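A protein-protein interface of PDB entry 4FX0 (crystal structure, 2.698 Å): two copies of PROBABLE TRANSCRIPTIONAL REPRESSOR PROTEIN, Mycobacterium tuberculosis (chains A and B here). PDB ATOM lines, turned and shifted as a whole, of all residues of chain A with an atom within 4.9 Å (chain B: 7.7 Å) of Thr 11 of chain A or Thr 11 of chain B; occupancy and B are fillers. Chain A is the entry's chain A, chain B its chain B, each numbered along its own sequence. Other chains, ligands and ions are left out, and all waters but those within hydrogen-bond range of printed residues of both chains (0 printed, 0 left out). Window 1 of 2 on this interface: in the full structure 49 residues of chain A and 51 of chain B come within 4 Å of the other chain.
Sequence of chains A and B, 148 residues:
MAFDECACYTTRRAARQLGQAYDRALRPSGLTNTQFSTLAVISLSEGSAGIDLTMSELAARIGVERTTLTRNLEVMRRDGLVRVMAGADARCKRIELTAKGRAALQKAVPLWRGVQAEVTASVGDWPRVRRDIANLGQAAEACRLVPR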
ATOM      1  N   ALA A   7     -24.030 -18.827   7.177  1.00  0.00           N
ATOM      2  CA  ALA A   7     -25.175 -18.927   6.283  1.00  0.00           C
ATOM      3  C   ALA A   7     -24.739 -18.880   4.826  1.00  0.00           C
ATOM      4  O   ALA A   7     -25.368 -19.488   3.959  1.00  0.00           O
ATOM      5  CB  ALA A   7     -26.168 -17.817   6.576  1.00  0.00           C
ATOM      6  N   CYS A   8     -23.660 -18.152   4.561  1.00  0.00           N
ATOM      7  CA  CYS A   8     -23.152 -18.020   3.204  1.00  0.00           C
ATOM      8  C   CYS A   8     -22.540 -19.337   2.737  1.00  0.00           C
ATOM      9  O   CYS A   8     -22.803 -19.795   1.625  1.00  0.00           O
ATOM     10  CB  CYS A   8     -22.123 -16.893   3.128  1.00  0.00           C
ATOM     11  SG  CYS A   8     -21.799 -16.305   1.453  1.00  0.00           S
ATOM     12  N   TYR A   9     -21.728 -19.943   3.597  1.00  0.00           N
ATOM     13  CA  TYR A   9     -21.109 -21.228   3.296  1.00  0.00           C
ATOM     14  C   TYR A   9     -22.151 -22.319   3.065  1.00  0.00           C
ATOM     15  O   TYR A   9     -22.189 -22.939   2.003  1.00  0.00           O
ATOM     16  CB  TYR A   9     -20.150 -21.637   4.419  1.00  0.00           C
ATOM     17  CG  TYR A   9     -19.851 -23.120   4.467  1.00  0.00           C
ATOM     18  CD1 TYR A   9     -19.214 -23.755   3.410  1.00  0.00           C
ATOM     19  CD2 TYR A   9     -20.202 -23.883   5.574  1.00  0.00           C
ATOM     20  CE1 TYR A   9     -18.940 -25.109   3.450  1.00  0.00           C
ATOM     21  CE2 TYR A   9     -19.930 -25.239   5.623  1.00  0.00           C
ATOM     22  CZ  TYR A   9     -19.299 -25.846   4.559  1.00  0.00           C
ATOM     23  OH  TYR A   9     -19.026 -27.194   4.604  1.00  0.00           O
ATOM     24  N   THR A  10     -22.998 -22.544   4.067  1.00  0.00           N
ATOM     25  CA  THR A  10     -24.007 -23.597   4.004  1.00  0.00           C
ATOM     26  C   THR A  10     -24.808 -23.527   2.709  1.00  0.00           C
ATOM     27  O   THR A  10     -25.010 -24.539   2.036  1.00  0.00           O
ATOM     28  CB  THR A  10     -24.981 -23.514   5.195  1.00  0.00           C
ATOM     29  OG1 THR A  10     -24.241 -23.478   6.422  1.00  0.00           O
ATOM     30  CG2 THR A  10     -25.913 -24.715   5.205  1.00  0.00           C
ATOM     31  N   THR A  11     -25.255 -22.326   2.366  1.00  0.00           N
ATOM     32  CA  THR A  11     -26.087 -22.127   1.185  1.00  0.00           C
ATOM     33  C   THR A  11     -25.301 -22.388  -0.094  1.00  0.00           C
ATOM     34  O   THR A  11     -25.748 -23.131  -0.967  1.00  0.00           O
ATOM     35  CB  THR A  11     -26.663 -20.701   1.139  1.00  0.00           C
ATOM     36  OG1 THR A  11     -27.099 -20.317   2.449  1.00  0.00           O
ATOM     37  CG2 THR A  11     -27.837 -20.633   0.178  1.00  0.00           C
ATOM     38  N   ARG A  12     -24.130 -21.772  -0.197  1.00  0.00           N
ATOM     39  CA  ARG A  12     -23.265 -21.938  -1.360  1.00  0.00           C
ATOM     40  C   ARG A  12     -22.984 -23.413  -1.641  1.00  0.00           C
ATOM     41  O   ARG A  12     -23.094 -23.870  -2.780  1.00  0.00           O
ATOM     42  CB  ARG A  12     -21.956 -21.174  -1.151  1.00  0.00           C
ATOM     43  CG  ARG A  12     -20.916 -21.371  -2.239  1.00  0.00           C
ATOM     44  CD  ARG A  12     -19.703 -20.500  -1.957  1.00  0.00           C
ATOM     45  NE  ARG A  12     -19.196 -20.715  -0.604  1.00  0.00           N
ATOM     46  CZ  ARG A  12     -18.525 -19.808   0.100  1.00  0.00           C
ATOM     47  NH1 ARG A  12     -18.279 -18.611  -0.415  1.00  0.00           N
ATOM     48  NH2 ARG A  12     -18.105 -20.097   1.325  1.00  0.00           N
ATOM     49  N   ARG A  13     -22.625 -24.154  -0.597  1.00  0.00           N
ATOM     50  CA  ARG A  13     -22.359 -25.582  -0.727  1.00  0.00           C
ATOM     51  C   ARG A  13     -23.607 -26.341  -1.174  1.00  0.00           C
ATOM     52  O   ARG A  13     -23.566 -27.100  -2.145  1.00  0.00           O
ATOM     53  CB  ARG A  13     -21.829 -26.154   0.590  1.00  0.00           C
ATOM     54  CG  ARG A  13     -21.659 -27.663   0.587  1.00  0.00           C
ATOM     55  CD  ARG A  13     -20.922 -28.139   1.827  1.00  0.00           C
ATOM     56  NE  ARG A  13     -20.879 -29.597   1.911  1.00  0.00           N
ATOM     57  CZ  ARG A  13     -20.051 -30.363   1.209  1.00  0.00           C
ATOM     58  NH1 ARG A  13     -19.195 -29.813   0.357  1.00  0.00           N
ATOM     59  NH2 ARG A  13     -20.083 -31.680   1.351  1.00  0.00           N
ATOM     60  N   ALA A  14     -24.712 -26.135  -0.464  1.00  0.00           N
ATOM     61  CA  ALA A  14     -25.973 -26.776  -0.821  1.00  0.00           C
ATOM     62  C   ALA A  14     -26.351 -26.457  -2.262  1.00  0.00           C
ATOM     63  O   ALA A  14     -26.769 -27.339  -3.013  1.00  0.00           O
ATOM     64  CB  ALA A  14     -27.079 -26.341   0.128  1.00  0.00           C
ATOM     65  N   ALA A  15     -26.194 -25.192  -2.641  1.00  0.00           N
ATOM     66  CA  ALA A  15     -26.531 -24.741  -3.988  1.00  0.00           C
ATOM     67  C   ALA A  15     -25.734 -25.506  -5.030  1.00  0.00           C
ATOM     68  O   ALA A  15     -26.274 -25.954  -6.042  1.00  0.00           O
ATOM     69  CB  ALA A  15     -26.278 -23.250  -4.124  1.00  0.00           C
ATOM     70  N   ARG A  16     -24.440 -25.653  -4.773  1.00  0.00           N
ATOM     71  CA  ARG A  16     -23.557 -26.366  -5.680  1.00  0.00           C
ATOM     72  C   ARG A  16     -24.008 -27.816  -5.833  1.00  0.00           C
ATOM     73  O   ARG A  16     -24.220 -28.294  -6.947  1.00  0.00           O
ATOM     74  CB  ARG A  16     -22.117 -26.290  -5.173  1.00  0.00           C
ATOM     75  CG  ARG A  16     -21.091 -26.914  -6.094  1.00  0.00           C
ATOM     76  CD  ARG A  16     -19.683 -26.507  -5.692  1.00  0.00           C
ATOM     77  NE  ARG A  16     -18.690 -27.477  -6.141  1.00  0.00           N
ATOM     78  CZ  ARG A  16     -18.289 -27.609  -7.401  1.00  0.00           C
ATOM     79  NH1 ARG A  16     -18.802 -26.832  -8.345  1.00  0.00           N
ATOM     80  NH2 ARG A  16     -17.380 -28.519  -7.717  1.00  0.00           N
ATOM     81  N   LEU A  18     -26.824 -29.119  -5.325  1.00  0.00           N
ATOM     82  CA  LEU A  18     -28.089 -29.124  -6.049  1.00  0.00           C
ATOM     83  C   LEU A  18     -27.877 -28.941  -7.548  1.00  0.00           C
ATOM     84  O   LEU A  18     -28.327 -29.760  -8.350  1.00  0.00           O
ATOM     85  CB  LEU A  18     -29.020 -28.038  -5.508  1.00  0.00           C
ATOM     86  CG  LEU A  18     -29.667 -28.332  -4.152  1.00  0.00           C
ATOM     87  CD1 LEU A  18     -30.291 -27.078  -3.563  1.00  0.00           C
ATOM     88  CD2 LEU A  18     -30.700 -29.442  -4.284  1.00  0.00           C
ATOM     89  N   ILE A 133     -35.243 -20.338   2.988  1.00  0.00           N
ATOM     90  CA  ILE A 133     -34.105 -20.064   2.116  1.00  0.00           C
ATOM     91  C   ILE A 133     -34.287 -18.743   1.373  1.00  0.00           C
ATOM     92  O   ILE A 133     -33.371 -17.920   1.318  1.00  0.00           O
ATOM     93  CB  ILE A 133     -33.879 -21.190   1.092  1.00  0.00           C
ATOM     94  CG1 ILE A 133     -33.616 -22.520   1.803  1.00  0.00           C
ATOM     95  CG2 ILE A 133     -32.714 -20.846   0.178  1.00  0.00           C
ATOM     96  CD1 ILE A 133     -33.330 -23.675   0.855  1.00  0.00           C
ATOM     97  N   LEU A 136     -33.865 -16.003   3.588  1.00  0.00           N
ATOM     98  CA  LEU A 136     -32.444 -15.858   3.858  1.00  0.00           C
ATOM     99  C   LEU A 136     -31.800 -14.942   2.823  1.00  0.00           C
ATOM    100  O   LEU A 136     -31.224 -13.909   3.168  1.00  0.00           O
ATOM    101  CB  LEU A 136     -31.770 -17.230   3.854  1.00  0.00           C
ATOM    102  CG  LEU A 136     -30.875 -17.558   5.050  1.00  0.00           C
ATOM    103  CD1 LEU A 136     -31.543 -17.150   6.355  1.00  0.00           C
ATOM    104  CD2 LEU A 136     -30.524 -19.040   5.055  1.00  0.00           C
ATOM    105  N   ASP B   4     -40.621 -21.197  -9.877  1.00  0.00           N
ATOM    106  CA  ASP B   4     -40.223 -20.339  -8.760  1.00  0.00           C
ATOM    107  C   ASP B   4     -39.770 -21.156  -7.560  1.00  0.00           C
ATOM    108  O   ASP B   4     -38.970 -20.705  -6.748  1.00  0.00           O
ATOM    109  CB  ASP B   4     -41.401 -19.441  -8.362  1.00  0.00           C
ATOM    110  CG  ASP B   4     -41.239 -18.826  -6.986  1.00  0.00           C
ATOM    111  OD1 ASP B   4     -40.104 -18.502  -6.616  1.00  0.00           O
ATOM    112  OD2 ASP B   4     -42.242 -18.693  -6.258  1.00  0.00           O
ATOM    113  N   GLU B   5     -40.286 -22.372  -7.456  1.00  0.00           N
ATOM    114  CA  GLU B   5     -40.024 -23.209  -6.295  1.00  0.00           C
ATOM    115  C   GLU B   5     -38.878 -24.205  -6.472  1.00  0.00           C
ATOM    116  O   GLU B   5     -38.553 -24.937  -5.535  1.00  0.00           O
ATOM    117  CB  GLU B   5     -41.293 -23.956  -5.873  1.00  0.00           C
ATOM    118  CG  GLU B   5     -42.328 -23.083  -5.191  1.00  0.00           C
ATOM    119  CD  GLU B   5     -43.300 -23.883  -4.345  1.00  0.00           C
ATOM    120  OE1 GLU B   5     -43.227 -25.129  -4.368  1.00  0.00           O
ATOM    121  OE2 GLU B   5     -44.136 -23.268  -3.651  1.00  0.00           O
ATOM    122  N   CYS B   6     -38.271 -24.242  -7.656  1.00  0.00           N
ATOM    123  CA  CYS B   6     -37.146 -25.144  -7.886  1.00  0.00           C
ATOM    124  C   CYS B   6     -36.106 -25.023  -6.772  1.00  0.00           C
ATOM    125  O   CYS B   6     -35.579 -23.940  -6.525  1.00  0.00           O
ATOM    126  CB  CYS B   6     -36.508 -24.872  -9.249  1.00  0.00           C
ATOM    127  SG  CYS B   6     -34.910 -25.679  -9.498  1.00  0.00           S
ATOM    128  N   ALA B   7     -35.821 -26.133  -6.094  1.00  0.00           N
ATOM    129  CA  ALA B   7     -34.834 -26.130  -5.014  1.00  0.00           C
ATOM    130  C   ALA B   7     -33.506 -25.536  -5.470  1.00  0.00           C
ATOM    131  O   ALA B   7     -32.970 -24.626  -4.837  1.00  0.00           O
ATOM    132  CB  ALA B   7     -34.624 -27.540  -4.466  1.00  0.00           C
ATOM    133  N   CYS B   8     -32.981 -26.063  -6.571  1.00  0.00           N
ATOM    134  CA  CYS B   8     -31.723 -25.587  -7.129  1.00  0.00           C
ATOM    135  C   CYS B   8     -31.781 -24.091  -7.407  1.00  0.00           C
ATOM    136  O   CYS B   8     -30.882 -23.344  -7.026  1.00  0.00           O
ATOM    137  CB  CYS B   8     -31.392 -26.344  -8.415  1.00  0.00           C
ATOM    138  SG  CYS B   8     -29.867 -25.805  -9.218  1.00  0.00           S
ATOM    139  N   TYR B   9     -32.847 -23.660  -8.074  1.00  0.00           N
ATOM    140  CA  TYR B   9     -33.012 -22.255  -8.427  1.00  0.00           C
ATOM    141  C   TYR B   9     -32.982 -21.343  -7.206  1.00  0.00           C
ATOM    142  O   TYR B   9     -32.144 -20.445  -7.111  1.00  0.00           O
ATOM    143  CB  TYR B   9     -34.314 -22.043  -9.200  1.00  0.00           C
ATOM    144  CG  TYR B   9     -34.824 -20.623  -9.137  1.00  0.00           C
ATOM    145  CD1 TYR B   9     -34.251 -19.623  -9.910  1.00  0.00           C
ATOM    146  CD2 TYR B   9     -35.877 -20.281  -8.298  1.00  0.00           C
ATOM    147  CE1 TYR B   9     -34.712 -18.321  -9.850  1.00  0.00           C
ATOM    148  CE2 TYR B   9     -36.345 -18.983  -8.232  1.00  0.00           C
ATOM    149  CZ  TYR B   9     -35.760 -18.007  -9.010  1.00  0.00           C
ATOM    150  OH  TYR B   9     -36.225 -16.714  -8.946  1.00  0.00           O
ATOM    151  N   THR B  10     -33.900 -21.576  -6.273  1.00  0.00           N
ATOM    152  CA  THR B  10     -34.035 -20.716  -5.102  1.00  0.00           C
ATOM    153  C   THR B  10     -32.757 -20.685  -4.273  1.00  0.00           C
ATOM    154  O   THR B  10     -32.297 -19.617  -3.864  1.00  0.00           O
ATOM    155  CB  THR B  10     -35.198 -21.160  -4.193  1.00  0.00           C
ATOM    156  OG1 THR B  10     -34.860 -22.390  -3.542  1.00  0.00           O
ATOM    157  CG2 THR B  10     -36.470 -21.347  -5.005  1.00  0.00           C
ATOM    158  N   THR B  11     -32.189 -21.861  -4.021  1.00  0.00           N
ATOM    159  CA  THR B  11     -30.971 -21.956  -3.226  1.00  0.00           C
ATOM    160  C   THR B  11     -29.829 -21.219  -3.916  1.00  0.00           C
ATOM    161  O   THR B  11     -29.064 -20.497  -3.274  1.00  0.00           O
ATOM    162  CB  THR B  11     -30.560 -23.419  -2.985  1.00  0.00           C
ATOM    163  OG1 THR B  11     -31.692 -24.170  -2.529  1.00  0.00           O
ATOM    164  CG2 THR B  11     -29.450 -23.492  -1.945  1.00  0.00           C
ATOM    165  N   ARG B  12     -29.721 -21.408  -5.228  1.00  0.00           N
ATOM    166  CA  ARG B  12     -28.710 -20.727  -6.027  1.00  0.00           C
ATOM    167  C   ARG B  12     -28.887 -19.215  -5.937  1.00  0.00           C
ATOM    168  O   ARG B  12     -27.948 -18.486  -5.614  1.00  0.00           O
ATOM    169  CB  ARG B  12     -28.799 -21.189  -7.484  1.00  0.00           C
ATOM    170  CG  ARG B  12     -27.873 -20.461  -8.446  1.00  0.00           C
ATOM    171  CD  ARG B  12     -27.923 -21.102  -9.825  1.00  0.00           C
ATOM    172  NE  ARG B  12     -29.291 -21.210 -10.323  1.00  0.00           N
ATOM    173  CZ  ARG B  12     -29.663 -21.991 -11.333  1.00  0.00           C
ATOM    174  NH1 ARG B  12     -28.767 -22.745 -11.956  1.00  0.00           N
ATOM    175  NH2 ARG B  12     -30.932 -22.023 -11.714  1.00  0.00           N
ATOM    176  N   ARG B  13     -30.103 -18.757  -6.219  1.00  0.00           N
ATOM    177  CA  ARG B  13     -30.446 -17.342  -6.142  1.00  0.00           C
ATOM    178  C   ARG B  13     -30.138 -16.770  -4.761  1.00  0.00           C
ATOM    179  O   ARG B  13     -29.539 -15.699  -4.637  1.00  0.00           O
ATOM    180  CB  ARG B  13     -31.925 -17.153  -6.485  1.00  0.00           C
ATOM    181  CG  ARG B  13     -32.461 -15.747  -6.276  1.00  0.00           C
ATOM    182  CD  ARG B  13     -33.845 -15.603  -6.897  1.00  0.00           C
ATOM    183  NE  ARG B  13     -34.502 -14.359  -6.509  1.00  0.00           N
ATOM    184  CZ  ARG B  13     -34.266 -13.179  -7.073  1.00  0.00           C
ATOM    185  NH1 ARG B  13     -33.377 -13.073  -8.052  1.00  0.00           N
ATOM    186  NH2 ARG B  13     -34.917 -12.103  -6.654  1.00  0.00           N
ATOM    187  N   ALA B  14     -30.546 -17.495  -3.723  1.00  0.00           N
ATOM    188  CA  ALA B  14     -30.280 -17.092  -2.347  1.00  0.00           C
ATOM    189  C   ALA B  14     -28.783 -16.967  -2.083  1.00  0.00           C
ATOM    190  O   ALA B  14     -28.293 -15.893  -1.734  1.00  0.00           O
ATOM    191  CB  ALA B  14     -30.907 -18.081  -1.376  1.00  0.00           C
ATOM    192  N   ALA B  15     -28.062 -18.072  -2.254  1.00  0.00           N
ATOM    193  CA  ALA B  15     -26.625 -18.107  -1.991  1.00  0.00           C
ATOM    194  C   ALA B  15     -25.907 -16.925  -2.627  1.00  0.00           C
ATOM    195  O   ALA B  15     -25.028 -16.320  -2.017  1.00  0.00           O
ATOM    196  CB  ALA B  15     -26.029 -19.416  -2.483  1.00  0.00           C
ATOM    197  N   ARG B  16     -26.289 -16.602  -3.858  1.00  0.00           N
ATOM    198  CA  ARG B  16     -25.683 -15.487  -4.572  1.00  0.00           C
ATOM    199  C   ARG B  16     -25.946 -14.167  -3.858  1.00  0.00           C
ATOM    200  O   ARG B  16     -25.021 -13.397  -3.602  1.00  0.00           O
ATOM    201  CB  ARG B  16     -26.192 -15.431  -6.013  1.00  0.00           C
ATOM    202  CG  ARG B  16     -25.755 -14.190  -6.764  1.00  0.00           C
ATOM    203  CD  ARG B  16     -26.051 -14.314  -8.245  1.00  0.00           C
ATOM    204  NE  ARG B  16     -26.034 -13.015  -8.911  1.00  0.00           N
ATOM    205  CZ  ARG B  16     -24.930 -12.323  -9.174  1.00  0.00           C
ATOM    206  NH1 ARG B  16     -23.744 -12.798  -8.821  1.00  0.00           N
ATOM    207  NH2 ARG B  16     -25.014 -11.149  -9.785  1.00  0.00           N
ATOM    208  N   GLN B  17     -27.209 -13.909  -3.532  1.00  0.00           N
ATOM    209  CA  GLN B  17     -27.570 -12.712  -2.780  1.00  0.00           C
ATOM    210  C   GLN B  17     -26.783 -12.642  -1.475  1.00  0.00           C
ATOM    211  O   GLN B  17     -26.363 -11.565  -1.050  1.00  0.00           O
ATOM    212  CB  GLN B  17     -29.071 -12.693  -2.488  1.00  0.00           C
ATOM    213  CG  GLN B  17     -29.944 -12.534  -3.720  1.00  0.00           C
ATOM    214  CD  GLN B  17     -31.389 -12.893  -3.450  1.00  0.00           C
ATOM    215  OE1 GLN B  17     -31.677 -13.800  -2.668  1.00  0.00           O
ATOM    216  NE2 GLN B  17     -32.308 -12.182  -4.093  1.00  0.00           N
ATOM    217  N   LEU B  18     -26.587 -13.796  -0.846  1.00  0.00           N
ATOM    218  CA  LEU B  18     -25.797 -13.882   0.379  1.00  0.00           C
ATOM    219  C   LEU B  18     -24.344 -13.506   0.116  1.00  0.00           C
ATOM    220  O   LEU B  18     -23.736 -12.757   0.885  1.00  0.00           O
ATOM    221  CB  LEU B  18     -25.875 -15.291   0.970  1.00  0.00           C
ATOM    222  CG  LEU B  18     -27.210 -15.675   1.611  1.00  0.00           C
ATOM    223  CD1 LEU B  18     -27.312 -17.180   1.799  1.00  0.00           C
ATOM    224  CD2 LEU B  18     -27.391 -14.948   2.935  1.00  0.00           C
ATOM    225  N   GLY B  19     -23.791 -14.032  -0.971  1.00  0.00           N
ATOM    226  CA  GLY B  19     -22.434 -13.705  -1.365  1.00  0.00           C
ATOM    227  C   GLY B  19     -22.252 -12.208  -1.526  1.00  0.00           C
ATOM    228  O   GLY B  19     -21.239 -11.648  -1.109  1.00  0.00           O
ATOM    229  N   TYR B  22     -22.522 -10.476   1.988  1.00  0.00           N
ATOM    230  CA  TYR B  22     -21.322 -10.831   2.739  1.00  0.00           C
ATOM    231  C   TYR B  22     -20.087 -10.118   2.194  1.00  0.00           C
ATOM    232  O   TYR B  22     -19.217  -9.698   2.956  1.00  0.00           O
ATOM    233  CB  TYR B  22     -21.125 -12.349   2.758  1.00  0.00           C
ATOM    234  CG  TYR B  22     -21.914 -13.037   3.852  1.00  0.00           C
ATOM    235  CD1 TYR B  22     -23.296 -12.922   3.914  1.00  0.00           C
ATOM    236  CD2 TYR B  22     -21.276 -13.797   4.823  1.00  0.00           C
ATOM    237  CE1 TYR B  22     -24.021 -13.542   4.913  1.00  0.00           C
ATOM    238  CE2 TYR B  22     -21.994 -14.424   5.827  1.00  0.00           C
ATOM    239  CZ  TYR B  22     -23.367 -14.292   5.866  1.00  0.00           C
ATOM    240  OH  TYR B  22     -24.088 -14.911   6.861  1.00  0.00           O
ATOM    241  N   GLY B  63     -16.897 -25.012  -0.740  1.00  0.00           N
ATOM    242  CA  GLY B  63     -18.070 -25.148  -1.585  1.00  0.00           C
ATOM    243  C   GLY B  63     -17.929 -24.444  -2.921  1.00  0.00           C
ATOM    244  O   GLY B  63     -18.909 -23.952  -3.479  1.00  0.00           O
ATOM    245  N   VAL B 119     -28.833 -11.510   8.884  1.00  0.00           N
ATOM    246  CA  VAL B 119     -29.435 -12.367   7.866  1.00  0.00           C
ATOM    247  C   VAL B 119     -30.208 -13.543   8.464  1.00  0.00           C
ATOM    248  O   VAL B 119     -31.301 -13.873   8.003  1.00  0.00           O
ATOM    249  CB  VAL B 119     -28.374 -12.883   6.868  1.00  0.00           C
ATOM    250  CG1 VAL B 119     -28.778 -14.232   6.297  1.00  0.00           C
ATOM    251  CG2 VAL B 119     -28.154 -11.865   5.758  1.00  0.00           C
ATOM    252  N   TRP B 126     -32.262 -20.546  13.204  1.00  0.00           N
ATOM    253  CA  TRP B 126     -31.186 -20.696  12.230  1.00  0.00           C
ATOM    254  C   TRP B 126     -30.560 -22.094  12.232  1.00  0.00           C
ATOM    255  O   TRP B 126     -30.400 -22.698  11.173  1.00  0.00           O
ATOM    256  CB  TRP B 126     -30.111 -19.623  12.422  1.00  0.00           C
ATOM    257  CG  TRP B 126     -28.864 -19.908  11.648  1.00  0.00           C
ATOM    258  CD1 TRP B 126     -27.588 -19.928  12.127  1.00  0.00           C
ATOM    259  CD2 TRP B 126     -28.776 -20.240  10.256  1.00  0.00           C
ATOM    260  NE1 TRP B 126     -26.709 -20.240  11.118  1.00  0.00           N
ATOM    261  CE2 TRP B 126     -27.414 -20.437   9.962  1.00  0.00           C
ATOM    262  CE3 TRP B 126     -29.718 -20.384   9.233  1.00  0.00           C
ATOM    263  CZ2 TRP B 126     -26.970 -20.771   8.682  1.00  0.00           C
ATOM    264  CZ3 TRP B 126     -29.275 -20.716   7.965  1.00  0.00           C
ATOM    265  CH2 TRP B 126     -27.913 -20.907   7.701  1.00  0.00           C
ATOM    266  N   ARG B 130     -30.410 -24.110   8.938  1.00  0.00           N
ATOM    267  CA  ARG B 130     -29.080 -24.420   8.438  1.00  0.00           C
ATOM    268  C   ARG B 130     -28.973 -25.912   8.171  1.00  0.00           C
ATOM    269  O   ARG B 130     -28.637 -26.339   7.065  1.00  0.00           O
ATOM    270  CB  ARG B 130     -28.014 -24.000   9.451  1.00  0.00           C
ATOM    271  CG  ARG B 130     -26.595 -24.043   8.905  1.00  0.00           C
ATOM    272  CD  ARG B 130     -25.577 -24.203  10.020  1.00  0.00           C
ATOM    273  NE  ARG B 130     -25.597 -25.552  10.576  1.00  0.00           N
ATOM    274  CZ  ARG B 130     -24.845 -26.552  10.128  1.00  0.00           C
ATOM    275  NH1 ARG B 130     -24.008 -26.356   9.118  1.00  0.00           N
ATOM    276  NH2 ARG B 130     -24.929 -27.749  10.693  1.00  0.00           N
ATOM    277  N   ILE B 133     -31.001 -27.015   5.156  1.00  0.00           N
ATOM    278  CA  ILE B 133     -30.333 -26.653   3.910  1.00  0.00           C
ATOM    279  C   ILE B 133     -29.167 -27.588   3.620  1.00  0.00           C
ATOM    280  O   ILE B 133     -29.038 -28.114   2.515  1.00  0.00           O
ATOM    281  CB  ILE B 133     -29.820 -25.200   3.950  1.00  0.00           C
ATOM    282  CG1 ILE B 133     -30.990 -24.228   4.122  1.00  0.00           C
ATOM    283  CG2 ILE B 133     -29.029 -24.880   2.689  1.00  0.00           C
ATOM    284  CD1 ILE B 133     -30.570 -22.780   4.276  1.00  0.00           C
ATOM    285  N   ALA B 134     -28.317 -27.789   4.622  1.00  0.00           N
ATOM    286  CA  ALA B 134     -27.183 -28.693   4.491  1.00  0.00           C
ATOM    287  C   ALA B 134     -27.659 -30.109   4.182  1.00  0.00           C
ATOM    288  O   ALA B 134     -27.122 -30.772   3.295  1.00  0.00           O
ATOM    289  CB  ALA B 134     -26.341 -28.676   5.757  1.00  0.00           C
ATOM    290  N   LEU B 136     -30.310 -30.800   2.757  1.00  0.00           N
ATOM    291  CA  LEU B 136     -30.834 -30.708   1.402  1.00  0.00           C
ATOM    292  C   LEU B 136     -29.700 -30.863   0.397  1.00  0.00           C
ATOM    293  O   LEU B 136     -29.845 -31.540  -0.622  1.00  0.00           O
ATOM    294  CB  LEU B 136     -31.540 -29.368   1.197  1.00  0.00           C
ATOM    295  CG  LEU B 136     -32.402 -29.234  -0.059  1.00  0.00           C
ATOM    296  CD1 LEU B 136     -33.539 -30.242  -0.034  1.00  0.00           C
ATOM    297  CD2 LEU B 136     -32.941 -27.817  -0.179  1.00  0.00           C
ATOM    298  N   GLY B 137     -28.567 -30.235   0.697  1.00  0.00           N
ATOM    299  CA  GLY B 137     -27.393 -30.324  -0.150  1.00  0.00           C
ATOM    300  C   GLY B 137     -26.825 -31.729  -0.204  1.00  0.00           C
ATOM    301  O   GLY B 137     -26.555 -32.253  -1.284  1.00  0.00           O
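Thr 11 of chain A touches its own counterpart, Thr 11 of chain B.
Thr 11 of chain A touches Ala 15 of chain B, and with the chains exchanged Ala 15 of chain A touches Thr 11 of chain B.
Among the printed residues, merely in contact across the chains: Ala 7 of chain A with Leu 18 of chain B (3.7 Å), Ala 7 of chain A with Tyr 22 of chain B (3.6 Å), Ala 7 of chain A with Trp 126 of chain B (3.5 Å), Cys 8 of chain A with Gly 19 of chain B (3.9 Å), Cys 8 of chain A with Tyr 22 of chain B (3.6 Å), Thr 10 of chain A with Arg 130 of chain B (3.5 Å), Thr 10 of chain A with Ala 134 of chain B (3.9 Å), Thr 11 of chain A with Thr 11 of chain B (3.7 Å), Thr 11 of chain A with Ala 15 of chain B (3.4 Å), Thr 11 of chain A with Leu 18 of chain B (3.2 Å), Arg 12 of chain A with Ala 15 of chain B (3.8 Å), Arg 12 of chain A with Gly 63 of chain B (3.5 Å), Ala 14 of chain A with Ile 133 of chain B (3.5 Å), Ala 14 of chain A with Gly 137 of chain B (3.9 Å), Ala 15 of chain A with Thr 11 of chain B (3.7 Å), Ala 15 of chain A with Arg 12 of chain B (3.99 Å), Arg 16 of chain A with Gly 63 of chain B (3.5 Å), Leu 18 of chain A with Ala 7 of chain B (3.8 Å), Leu 18 of chain A with Cys 8 of chain B (3.99 Å), Leu 18 of chain A with Thr 11 of chain B (3.4 Å), Ile 133 of chain A with Thr 11 of chain B (3.8 Å), Ile 133 of chain A with Ala 14 of chain B (3.7 Å), Ile 133 of chain A with Ile 133 of chain B (3.9 Å), Leu 136 of chain A with Leu 18 of chain B (3.98 Å), Leu 136 of chain A with Val 119 of chain B (3.7 Å), Leu 136 of chain A with Trp 126 of chain B (3.6 Å) and Leu 136 of chain A with Ile 133 of chain B (3.8 Å).
Of chain B, only Thr 11 (3.7 Å), Ala 15 (3.4 Å) and Leu 18 (3.2 Å) come within 4 Å of Thr 11 of chain A.
Thr 11 of chain B touches four residues of chain A.
Of the printed residues of chain B, Arg 12 of chain A touches Ala 15 and Gly 63.
Of the printed residues of chain A, Arg 130 of chain B touches Thr 10.
Arg 13 of chain B touches none of the printed residues of chain A.
The nearest printed residue of chain B that does not touch Thr 11 of chain A is Ala 14 of chain B (4.3 Å).
The nearest residue of chain A that does not touch Thr 11 of chain B is Ala 14 of chain A (4.2 Å).
The nearest printed residue of chain A that does not touch Ala 14 of chain B is Thr 11 of chain A (4.3 Å).
Hydrophobic or aromatic side chains of chain A that line the printed part of chain B: Ala 7, Ala 14, Ala 15, Leu 18, Ile 133 and Leu 136.
Along chain A the printed residues that touch a printed residue of chain B span positions 7 to 136.
Of the 25 printed residues of chain B, 16 touch a printed residue of chain A.
Hydrophobic or aromatic side chains of chain B within 4 Å of the printed part of chain A: Ala 14, Ala 15, Leu 18, Tyr 22, Val 119, Trp 126 and Ile 133.
Among the printed residues, 27 pairs touch across the chains.
Among the printed residues, no Asp or Glu carboxylate lies within 4 Å of a Lys or Arg side-chain nitrogen of the other chain.
The backbone carbonyl oxygen of Ala 7 of chain B lies within hydrogen-bond range of the side-chain hydroxyl of Thr 10 of chain B, 3.2 Å away.
The side-chain hydroxyl (OG1) of Thr 11 of chain B lies within hydrogen-bond range of the backbone carbonyl oxygen (O) of Ala 7 of chain B, at 2.7 Å.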
